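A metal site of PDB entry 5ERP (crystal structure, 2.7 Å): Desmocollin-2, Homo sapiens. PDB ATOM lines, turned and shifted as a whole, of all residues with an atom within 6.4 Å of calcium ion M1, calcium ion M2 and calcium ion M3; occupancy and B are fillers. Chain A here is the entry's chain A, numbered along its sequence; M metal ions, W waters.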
ATOM      1  N   GLU A  19      11.145 -14.614   1.231  1.00  0.00           N
ATOM      2  CA  GLU A  19      11.671 -14.332   2.560  1.00  0.00           C
ATOM      3  C   GLU A  19      10.614 -14.647   3.618  1.00  0.00           C
ATOM      4  O   GLU A  19       9.416 -14.707   3.310  1.00  0.00           O
ATOM      5  CB  GLU A  19      12.116 -12.872   2.664  1.00  0.00           C
ATOM      6  CG  GLU A  19      10.988 -11.875   2.443  1.00  0.00           C
ATOM      7  CD  GLU A  19      11.448 -10.438   2.606  1.00  0.00           C
ATOM      8  OE1 GLU A  19      12.323 -10.171   3.462  1.00  0.00           O
ATOM      9  OE2 GLU A  19      10.931  -9.576   1.877  1.00  0.00           O
ATOM     10  N   ASN A  20      11.064 -14.828   4.851  1.00  0.00           N
ATOM     11  CA  ASN A  20      10.181 -15.120   5.974  1.00  0.00           C
ATOM     12  C   ASN A  20       9.414 -16.434   5.815  1.00  0.00           C
ATOM     13  O   ASN A  20       8.445 -16.682   6.537  1.00  0.00           O
ATOM     14  CB  ASN A  20       9.193 -13.976   6.192  1.00  0.00           C
ATOM     15  CG  ASN A  20       9.869 -12.628   6.273  1.00  0.00           C
ATOM     16  OD1 ASN A  20      11.046 -12.546   6.635  1.00  0.00           O
ATOM     17  ND2 ASN A  20       9.133 -11.565   5.958  1.00  0.00           N
ATOM     18  N   LEU A  76      15.284 -15.770   6.859  1.00  0.00           N
ATOM     19  CA  LEU A  76      15.716 -15.291   5.553  1.00  0.00           C
ATOM     20  C   LEU A  76      15.144 -13.891   5.335  1.00  0.00           C
ATOM     21  O   LEU A  76      13.932 -13.699   5.392  1.00  0.00           O
ATOM     22  CB  LEU A  76      15.249 -16.244   4.455  1.00  0.00           C
ATOM     23  CG  LEU A  76      15.824 -17.657   4.520  1.00  0.00           C
ATOM     24  CD1 LEU A  76      14.831 -18.660   3.953  1.00  0.00           C
ATOM     25  CD2 LEU A  76      17.161 -17.716   3.789  1.00  0.00           C
ATOM     26  N   ASP A  77      16.028 -12.935   5.076  1.00  0.00           N
ATOM     27  CA  ASP A  77      15.634 -11.535   4.979  1.00  0.00           C
ATOM     28  C   ASP A  77      16.246 -10.878   3.751  1.00  0.00           C
ATOM     29  O   ASP A  77      17.466 -10.695   3.678  1.00  0.00           O
ATOM     30  CB  ASP A  77      16.036 -10.782   6.246  1.00  0.00           C
ATOM     31  CG  ASP A  77      15.384  -9.412   6.349  1.00  0.00           C
ATOM     32  OD1 ASP A  77      14.483  -9.114   5.548  1.00  0.00           O
ATOM     33  OD2 ASP A  77      15.775  -8.632   7.244  1.00  0.00           O
ATOM     34  N   ARG A  78      15.398 -10.529   2.796  1.00  0.00           N
ATOM     35  CA  ARG A  78      15.831  -9.984   1.519  1.00  0.00           C
ATOM     36  C   ARG A  78      16.573  -8.662   1.702  1.00  0.00           C
ATOM     37  O   ARG A  78      17.495  -8.350   0.948  1.00  0.00           O
ATOM     38  CB  ARG A  78      14.617  -9.777   0.596  1.00  0.00           C
ATOM     39  CG  ARG A  78      14.977  -9.722  -0.886  1.00  0.00           C
ATOM     40  CD  ARG A  78      14.097  -8.762  -1.691  1.00  0.00           C
ATOM     41  NE  ARG A  78      14.787  -7.514  -1.984  1.00  0.00           N
ATOM     42  CZ  ARG A  78      14.585  -6.352  -1.361  1.00  0.00           C
ATOM     43  NH1 ARG A  78      13.676  -6.245  -0.401  1.00  0.00           N
ATOM     44  NH2 ARG A  78      15.299  -5.303  -1.725  1.00  0.00           N
ATOM     45  N   GLU A  79      16.170  -7.891   2.709  1.00  0.00           N
ATOM     46  CA  GLU A  79      16.749  -6.573   2.962  1.00  0.00           C
ATOM     47  C   GLU A  79      18.124  -6.650   3.625  1.00  0.00           C
ATOM     48  O   GLU A  79      18.822  -5.650   3.734  1.00  0.00           O
ATOM     49  CB  GLU A  79      15.790  -5.736   3.816  1.00  0.00           C
ATOM     50  CG  GLU A  79      14.564  -5.226   3.052  1.00  0.00           C
ATOM     51  CD  GLU A  79      13.483  -6.279   2.870  1.00  0.00           C
ATOM     52  OE1 GLU A  79      13.482  -7.281   3.618  1.00  0.00           O
ATOM     53  OE2 GLU A  79      12.632  -6.106   1.969  1.00  0.00           O
ATOM     54  N   LEU A  80      18.498  -7.849   4.085  1.00  0.00           N
ATOM     55  CA  LEU A  80      19.835  -8.067   4.663  1.00  0.00           C
ATOM     56  C   LEU A  80      20.711  -8.829   3.673  1.00  0.00           C
ATOM     57  O   LEU A  80      21.828  -8.407   3.377  1.00  0.00           O
ATOM     58  CB  LEU A  80      19.737  -8.833   5.981  1.00  0.00           C
ATOM     59  CG  LEU A  80      19.072  -8.097   7.156  1.00  0.00           C
ATOM     60  CD1 LEU A  80      18.881  -9.034   8.340  1.00  0.00           C
ATOM     61  CD2 LEU A  80      19.900  -6.887   7.566  1.00  0.00           C
ATOM     62  N   ASP A 111      13.065 -13.808  -2.895  1.00  0.00           N
ATOM     63  CA  ASP A 111      12.043 -12.964  -3.469  1.00  0.00           C
ATOM     64  C   ASP A 111      11.484 -12.055  -2.387  1.00  0.00           C
ATOM     65  O   ASP A 111      11.609 -12.344  -1.194  1.00  0.00           O
ATOM     66  CB  ASP A 111      10.936 -13.814  -4.089  1.00  0.00           C
ATOM     67  CG  ASP A 111      10.325 -13.187  -5.326  1.00  0.00           C
ATOM     68  OD1 ASP A 111      10.270 -11.941  -5.404  1.00  0.00           O
ATOM     69  OD2 ASP A 111       9.894 -13.940  -6.213  1.00  0.00           O
ATOM     70  N   ASP A 112      10.857 -10.951  -2.790  1.00  0.00           N
ATOM     71  CA  ASP A 112      10.395  -9.945  -1.850  1.00  0.00           C
ATOM     72  C   ASP A 112       8.935 -10.161  -1.438  1.00  0.00           C
ATOM     73  O   ASP A 112       8.110 -10.592  -2.242  1.00  0.00           O
ATOM     74  CB  ASP A 112      10.556  -8.547  -2.451  1.00  0.00           C
ATOM     75  CG  ASP A 112      10.242  -7.435  -1.468  1.00  0.00           C
ATOM     76  OD1 ASP A 112      10.854  -7.429  -0.381  1.00  0.00           O
ATOM     77  OD2 ASP A 112       9.389  -6.580  -1.790  1.00  0.00           O
ATOM     78  N   VAL A 113       8.648  -9.871  -0.171  1.00  0.00           N
ATOM     79  CA  VAL A 113       7.271  -9.771   0.315  1.00  0.00           C
ATOM     80  C   VAL A 113       7.130  -8.425   1.001  1.00  0.00           C
ATOM     81  O   VAL A 113       8.127  -7.834   1.427  1.00  0.00           O
ATOM     82  CB  VAL A 113       6.889 -10.925   1.280  1.00  0.00           C
ATOM     83  CG1 VAL A 113       7.255 -12.282   0.687  1.00  0.00           C
ATOM     84  CG2 VAL A 113       7.551 -10.742   2.636  1.00  0.00           C
ATOM     85  N   ASN A 114       5.902  -7.925   1.111  1.00  0.00           N
ATOM     86  CA  ASN A 114       5.655  -6.603   1.664  1.00  0.00           C
ATOM     87  C   ASN A 114       5.672  -6.608   3.197  1.00  0.00           C
ATOM     88  O   ASN A 114       4.622  -6.775   3.824  1.00  0.00           O
ATOM     89  CB  ASN A 114       4.311  -6.067   1.150  1.00  0.00           C
ATOM     90  CG  ASN A 114       4.008  -4.655   1.632  1.00  0.00           C
ATOM     91  OD1 ASN A 114       4.906  -3.840   1.808  1.00  0.00           O
ATOM     92  ND2 ASN A 114       2.735  -4.371   1.825  1.00  0.00           N
ATOM     93  N   ASP A 115       6.848  -6.441   3.782  1.00  0.00           N
ATOM     94  CA  ASP A 115       6.994  -6.467   5.243  1.00  0.00           C
ATOM     95  C   ASP A 115       7.579  -5.175   5.803  1.00  0.00           C
ATOM     96  O   ASP A 115       7.926  -5.111   6.989  1.00  0.00           O
ATOM     97  CB  ASP A 115       7.851  -7.665   5.672  1.00  0.00           C
ATOM     98  CG  ASP A 115       9.193  -7.722   4.962  1.00  0.00           C
ATOM     99  OD1 ASP A 115       9.446  -6.894   4.072  1.00  0.00           O
ATOM    100  OD2 ASP A 115       9.984  -8.615   5.309  1.00  0.00           O
ATOM    101  N   HIS A 116       7.699  -4.154   4.963  1.00  0.00           N
ATOM    102  CA  HIS A 116       7.964  -2.784   5.429  1.00  0.00           C
ATOM    103  C   HIS A 116       6.851  -1.856   4.975  1.00  0.00           C
ATOM    104  O   HIS A 116       6.630  -1.675   3.781  1.00  0.00           O
ATOM    105  CB  HIS A 116       9.312  -2.270   4.906  1.00  0.00           C
ATOM    106  CG  HIS A 116      10.501  -2.992   5.452  1.00  0.00           C
ATOM    107  ND1 HIS A 116      11.062  -4.088   4.831  1.00  0.00           N
ATOM    108  CD2 HIS A 116      11.250  -2.759   6.557  1.00  0.00           C
ATOM    109  CE1 HIS A 116      12.095  -4.504   5.536  1.00  0.00           C
ATOM    110  NE2 HIS A 116      12.230  -3.719   6.594  1.00  0.00           N
ATOM    111  N   LEU A 117       6.141  -1.249   5.926  1.00  0.00           N
ATOM    112  CA  LEU A 117       5.098  -0.294   5.586  1.00  0.00           C
ATOM    113  C   LEU A 117       5.734   1.013   5.156  1.00  0.00           C
ATOM    114  O   LEU A 117       6.744   1.432   5.742  1.00  0.00           O
ATOM    115  CB  LEU A 117       4.153  -0.056   6.763  1.00  0.00           C
ATOM    116  CG  LEU A 117       3.380  -1.283   7.241  1.00  0.00           C
ATOM    117  CD1 LEU A 117       2.837  -1.055   8.642  1.00  0.00           C
ATOM    118  CD2 LEU A 117       2.228  -1.573   6.278  1.00  0.00           C
ATOM    119  N   PRO A 118       5.169   1.686   4.140  1.00  0.00           N
ATOM    120  CA  PRO A 118       5.767   2.950   3.720  1.00  0.00           C
ATOM    121  C   PRO A 118       5.440   4.055   4.712  1.00  0.00           C
ATOM    122  O   PRO A 118       4.342   4.098   5.258  1.00  0.00           O
ATOM    123  CB  PRO A 118       5.128   3.203   2.361  1.00  0.00           C
ATOM    124  CG  PRO A 118       3.782   2.575   2.469  1.00  0.00           C
ATOM    125  CD  PRO A 118       3.932   1.392   3.398  1.00  0.00           C
ATOM    126  N   ASP A 145      10.408   3.275   1.923  1.00  0.00           N
ATOM    127  CA  ASP A 145       9.951   1.895   1.864  1.00  0.00           C
ATOM    128  C   ASP A 145      11.136   1.008   1.515  1.00  0.00           C
ATOM    129  O   ASP A 145      11.739   1.159   0.452  1.00  0.00           O
ATOM    130  CB  ASP A 145       8.827   1.725   0.843  1.00  0.00           C
ATOM    131  CG  ASP A 145       8.053   0.434   1.032  1.00  0.00           C
ATOM    132  OD1 ASP A 145       8.683  -0.620   1.229  1.00  0.00           O
ATOM    133  OD2 ASP A 145       6.807   0.482   0.984  1.00  0.00           O
ATOM    134  N   LYS A 146      11.449   0.080   2.410  1.00  0.00           N
ATOM    135  CA  LYS A 146      12.645  -0.737   2.269  1.00  0.00           C
ATOM    136  C   LYS A 146      12.420  -1.970   1.401  1.00  0.00           C
ATOM    137  O   LYS A 146      13.355  -2.740   1.163  1.00  0.00           O
ATOM    138  CB  LYS A 146      13.146  -1.150   3.649  1.00  0.00           C
ATOM    139  CG  LYS A 146      13.858  -0.027   4.372  1.00  0.00           C
ATOM    140  CD  LYS A 146      13.940  -0.253   5.867  1.00  0.00           C
ATOM    141  CE  LYS A 146      14.589   0.919   6.578  1.00  0.00           C
ATOM    142  NZ  LYS A 146      15.953   1.202   6.039  1.00  0.00           N
ATOM    143  N   ASP A 147      11.200  -2.146   0.911  1.00  0.00           N
ATOM    144  CA  ASP A 147      10.906  -3.304   0.066  1.00  0.00           C
ATOM    145  C   ASP A 147      11.474  -3.075  -1.331  1.00  0.00           C
ATOM    146  O   ASP A 147      12.062  -2.033  -1.607  1.00  0.00           O
ATOM    147  CB  ASP A 147       9.396  -3.562   0.008  1.00  0.00           C
ATOM    148  CG  ASP A 147       8.845  -4.051   1.332  1.00  0.00           C
ATOM    149  OD1 ASP A 147       9.558  -4.794   2.040  1.00  0.00           O
ATOM    150  OD2 ASP A 147       7.691  -3.703   1.664  1.00  0.00           O
ATOM    151  N   LEU A 148      11.289  -4.058  -2.196  1.00  0.00           N
ATOM    152  CA  LEU A 148      11.939  -4.073  -3.499  1.00  0.00           C
ATOM    153  C   LEU A 148      11.333  -3.060  -4.473  1.00  0.00           C
ATOM    154  O   LEU A 148      10.126  -3.066  -4.711  1.00  0.00           O
ATOM    155  CB  LEU A 148      11.885  -5.476  -4.090  1.00  0.00           C
ATOM    156  CG  LEU A 148      12.485  -5.661  -5.487  1.00  0.00           C
ATOM    157  CD1 LEU A 148      13.951  -5.282  -5.492  1.00  0.00           C
ATOM    158  CD2 LEU A 148      12.293  -7.094  -5.947  1.00  0.00           C
ATOM    159  N   ALA A 152       4.597  -3.939  -6.297  1.00  0.00           N
ATOM    160  CA  ALA A 152       3.402  -3.602  -5.536  1.00  0.00           C
ATOM    161  C   ALA A 152       3.678  -3.570  -4.027  1.00  0.00           C
ATOM    162  O   ALA A 152       2.851  -3.084  -3.256  1.00  0.00           O
ATOM    163  CB  ALA A 152       2.285  -4.596  -5.840  1.00  0.00           C
ATOM    164  N   ASN A 153       4.820  -4.100  -3.620  1.00  0.00           N
ATOM    165  CA  ASN A 153       5.225  -4.074  -2.218  1.00  0.00           C
ATOM    166  C   ASN A 153       5.925  -2.771  -1.874  1.00  0.00           C
ATOM    167  O   ASN A 153       6.218  -2.507  -0.706  1.00  0.00           O
ATOM    168  CB  ASN A 153       6.157  -5.242  -1.914  1.00  0.00           C
ATOM    169  CG  ASN A 153       5.549  -6.585  -2.230  1.00  0.00           C
ATOM    170  OD1 ASN A 153       4.328  -6.749  -2.233  1.00  0.00           O
ATOM    171  ND2 ASN A 153       6.399  -7.566  -2.530  1.00  0.00           N
ATOM    172  N   TRP A 154       6.184  -1.953  -2.886  1.00  0.00           N
ATOM    173  CA  TRP A 154       6.990  -0.747  -2.729  1.00  0.00           C
ATOM    174  C   TRP A 154       6.231   0.534  -3.049  1.00  0.00           C
ATOM    175  O   TRP A 154       6.193   1.463  -2.232  1.00  0.00           O
ATOM    176  CB  TRP A 154       8.219  -0.836  -3.634  1.00  0.00           C
ATOM    177  CG  TRP A 154       9.068   0.388  -3.649  1.00  0.00           C
ATOM    178  CD1 TRP A 154       9.967   0.778  -2.697  1.00  0.00           C
ATOM    179  CD2 TRP A 154       9.124   1.380  -4.675  1.00  0.00           C
ATOM    180  NE1 TRP A 154      10.572   1.946  -3.066  1.00  0.00           N
ATOM    181  CE2 TRP A 154      10.080   2.343  -4.275  1.00  0.00           C
ATOM    182  CE3 TRP A 154       8.473   1.544  -5.896  1.00  0.00           C
ATOM    183  CZ2 TRP A 154      10.382   3.456  -5.052  1.00  0.00           C
ATOM    184  CZ3 TRP A 154       8.773   2.648  -6.671  1.00  0.00           C
ATOM    185  CH2 TRP A 154       9.720   3.585  -6.248  1.00  0.00           C
ATOM    186  N   ARG A 155       5.629   0.594  -4.229  1.00  0.00           N
ATOM    187  CA  ARG A 155       5.030   1.833  -4.724  1.00  0.00           C
ATOM    188  C   ARG A 155       3.831   2.263  -3.898  1.00  0.00           C
ATOM    189  O   ARG A 155       3.040   1.434  -3.445  1.00  0.00           O
ATOM    190  CB  ARG A 155       4.624   1.675  -6.186  1.00  0.00           C
ATOM    191  CG  ARG A 155       3.534   0.664  -6.439  1.00  0.00           C
ATOM    192  CD  ARG A 155       3.177   0.618  -7.922  1.00  0.00           C
ATOM    193  NE  ARG A 155       3.210  -0.739  -8.462  1.00  0.00           N
ATOM    194  CZ  ARG A 155       4.213  -1.252  -9.159  1.00  0.00           C
ATOM    195  NH1 ARG A 155       5.307  -0.535  -9.422  1.00  0.00           N
ATOM    196  NH2 ARG A 155       4.133  -2.494  -9.599  1.00  0.00           N
ATOM    197  N   ASN A 204       0.854   0.689   0.393  1.00  0.00           N
ATOM    198  CA  ASN A 204       1.316   0.086  -0.861  1.00  0.00           C
ATOM    199  C   ASN A 204       0.115  -0.425  -1.647  1.00  0.00           C
ATOM    200  O   ASN A 204      -0.993  -0.506  -1.122  1.00  0.00           O
ATOM    201  CB  ASN A 204       2.281  -1.062  -0.595  1.00  0.00           C
ATOM    202  CG  ASN A 204       3.428  -0.666   0.316  1.00  0.00           C
ATOM    203  OD1 ASN A 204       3.566  -1.207   1.413  1.00  0.00           O
ATOM    204  ND2 ASN A 204       4.261   0.258  -0.135  1.00  0.00           N
ATOM    205  N   PHE A 208       0.037  -5.393   3.578  1.00  0.00           N
ATOM    206  CA  PHE A 208       1.163  -5.747   4.448  1.00  0.00           C
ATOM    207  C   PHE A 208       1.231  -7.280   4.541  1.00  0.00           C
ATOM    208  O   PHE A 208       0.211  -7.941   4.310  1.00  0.00           O
ATOM    209  CB  PHE A 208       0.971  -5.126   5.840  1.00  0.00           C
ATOM    210  CG  PHE A 208       2.187  -5.155   6.720  1.00  0.00           C
ATOM    211  CD1 PHE A 208       3.444  -4.840   6.214  1.00  0.00           C
ATOM    212  CD2 PHE A 208       2.085  -5.488   8.060  1.00  0.00           C
ATOM    213  CE1 PHE A 208       4.561  -4.852   7.039  1.00  0.00           C
ATOM    214  CE2 PHE A 208       3.203  -5.512   8.877  1.00  0.00           C
ATOM    215  CZ  PHE A 208       4.441  -5.194   8.366  1.00  0.00           C
HETATM  216 CA    CA M   1      10.517  -7.107   1.982  1.00  0.00          CA
HETATM  217 CA    CA M   2      12.297  -8.515   5.299  1.00  0.00          CA
HETATM  218 CA    CA M   3       6.284  -1.849   1.535  1.00  0.00          CA
HETATM  219  O   HOH W   1      12.566  -6.943   7.164  1.00  0.00           O
HETATM  220  O   HOH W   2      12.062 -10.468   6.622  1.00  0.00           O
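The guanidinium group of Arg 78 sits close to the side-chain carboxylate of Asp 112 (3.1 Å). The side-chain carboxylate (OE2) of Glu 79 sits close to the guanidinium group (NH1) of Arg 78 (2.6 Å). The side-chain carboxylate (OD2) of Asp 115 sits close to the side-chain amide nitrogen (ND2) of Asn 20 (3.1 Å). The backbone NH of Arg 78 sits close to the side-chain carboxylate of Glu 19 (3.2 Å). The side-chain amide nitrogen of Asn 114 lies close to the backbone NH of Phe 208. The side-chain carboxylate (OD2) of Asp 112 lies within hydrogen-bond range of the backbone NH (N) of Leu 148, 3.2 Å away. ND2 of Asn 153 lies within hydrogen-bond range of OD2 of Asp 112 (3.2 Å). The backbone carbonyl oxygen of Trp 154 sits at hydrogen-bond distance from the side-chain amide nitrogen of Asn 204, 3.1 Å away.
Six residues have an atom within 4 Å of calcium ion M1: Glu 19, Glu 79, Asp 112, Val 113, Asp 115 and Asp 147. The nearest printed residue that does not touch calcium ion M1 is Arg 78 (4.05 Å).
Within 4 Å of calcium ion M3: Asn 114, His 116, Asp 145, Asp 147, Asn 153 and Asn 204.
Calcium ion M1 is bound by the side-chain carboxylate of Glu 79, the side-chain carboxylate of Asp 115, the side-chain carboxylate of Asp 112, the side-chain carboxylate of Glu 19, the side-chain carboxylate of Asp 147 and the backbone carbonyl oxygen of Val 113. Calcium ion M1 has six donor atoms within binding distance.
Calcium ion M2 is bound by the side-chain carboxylate (OD1) of Asp 77 (2.3 Å). OD2 of Asp 115 binds calcium ion M2 (2.3 Å). Calcium ion M2 is bound by water W2 (2.4 Å). The side-chain carboxylate (OE1) of Glu 79 binds calcium ion M2 (2.4 Å). Calcium ion M2 is bound by water W1 (2.5 Å). Calcium ion M2 is bound by OE1 of Glu 19. Calcium ion M2 has six donor atoms within binding distance.
Calcium ion M3 is bound by the backbone carbonyl oxygen (O) of His 116 (2.3 Å), the side-chain carboxylate (OD2) of Asp 147 (2.3 Å), the backbone carbonyl oxygen (O) of Asn 153 (2.3 Å), the side-chain amide oxygen (OD1) of Asn 114 (2.4 Å), the side-chain carboxylate (OD2) of Asp 145 (2.5 Å), the side-chain carboxylate (OD1) of Asp 145 (2.7 Å) and the side-chain amide oxygen (OD1) of Asn 204 (2.8 Å). Calcium ion M3 has seven donor atoms within binding distance.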
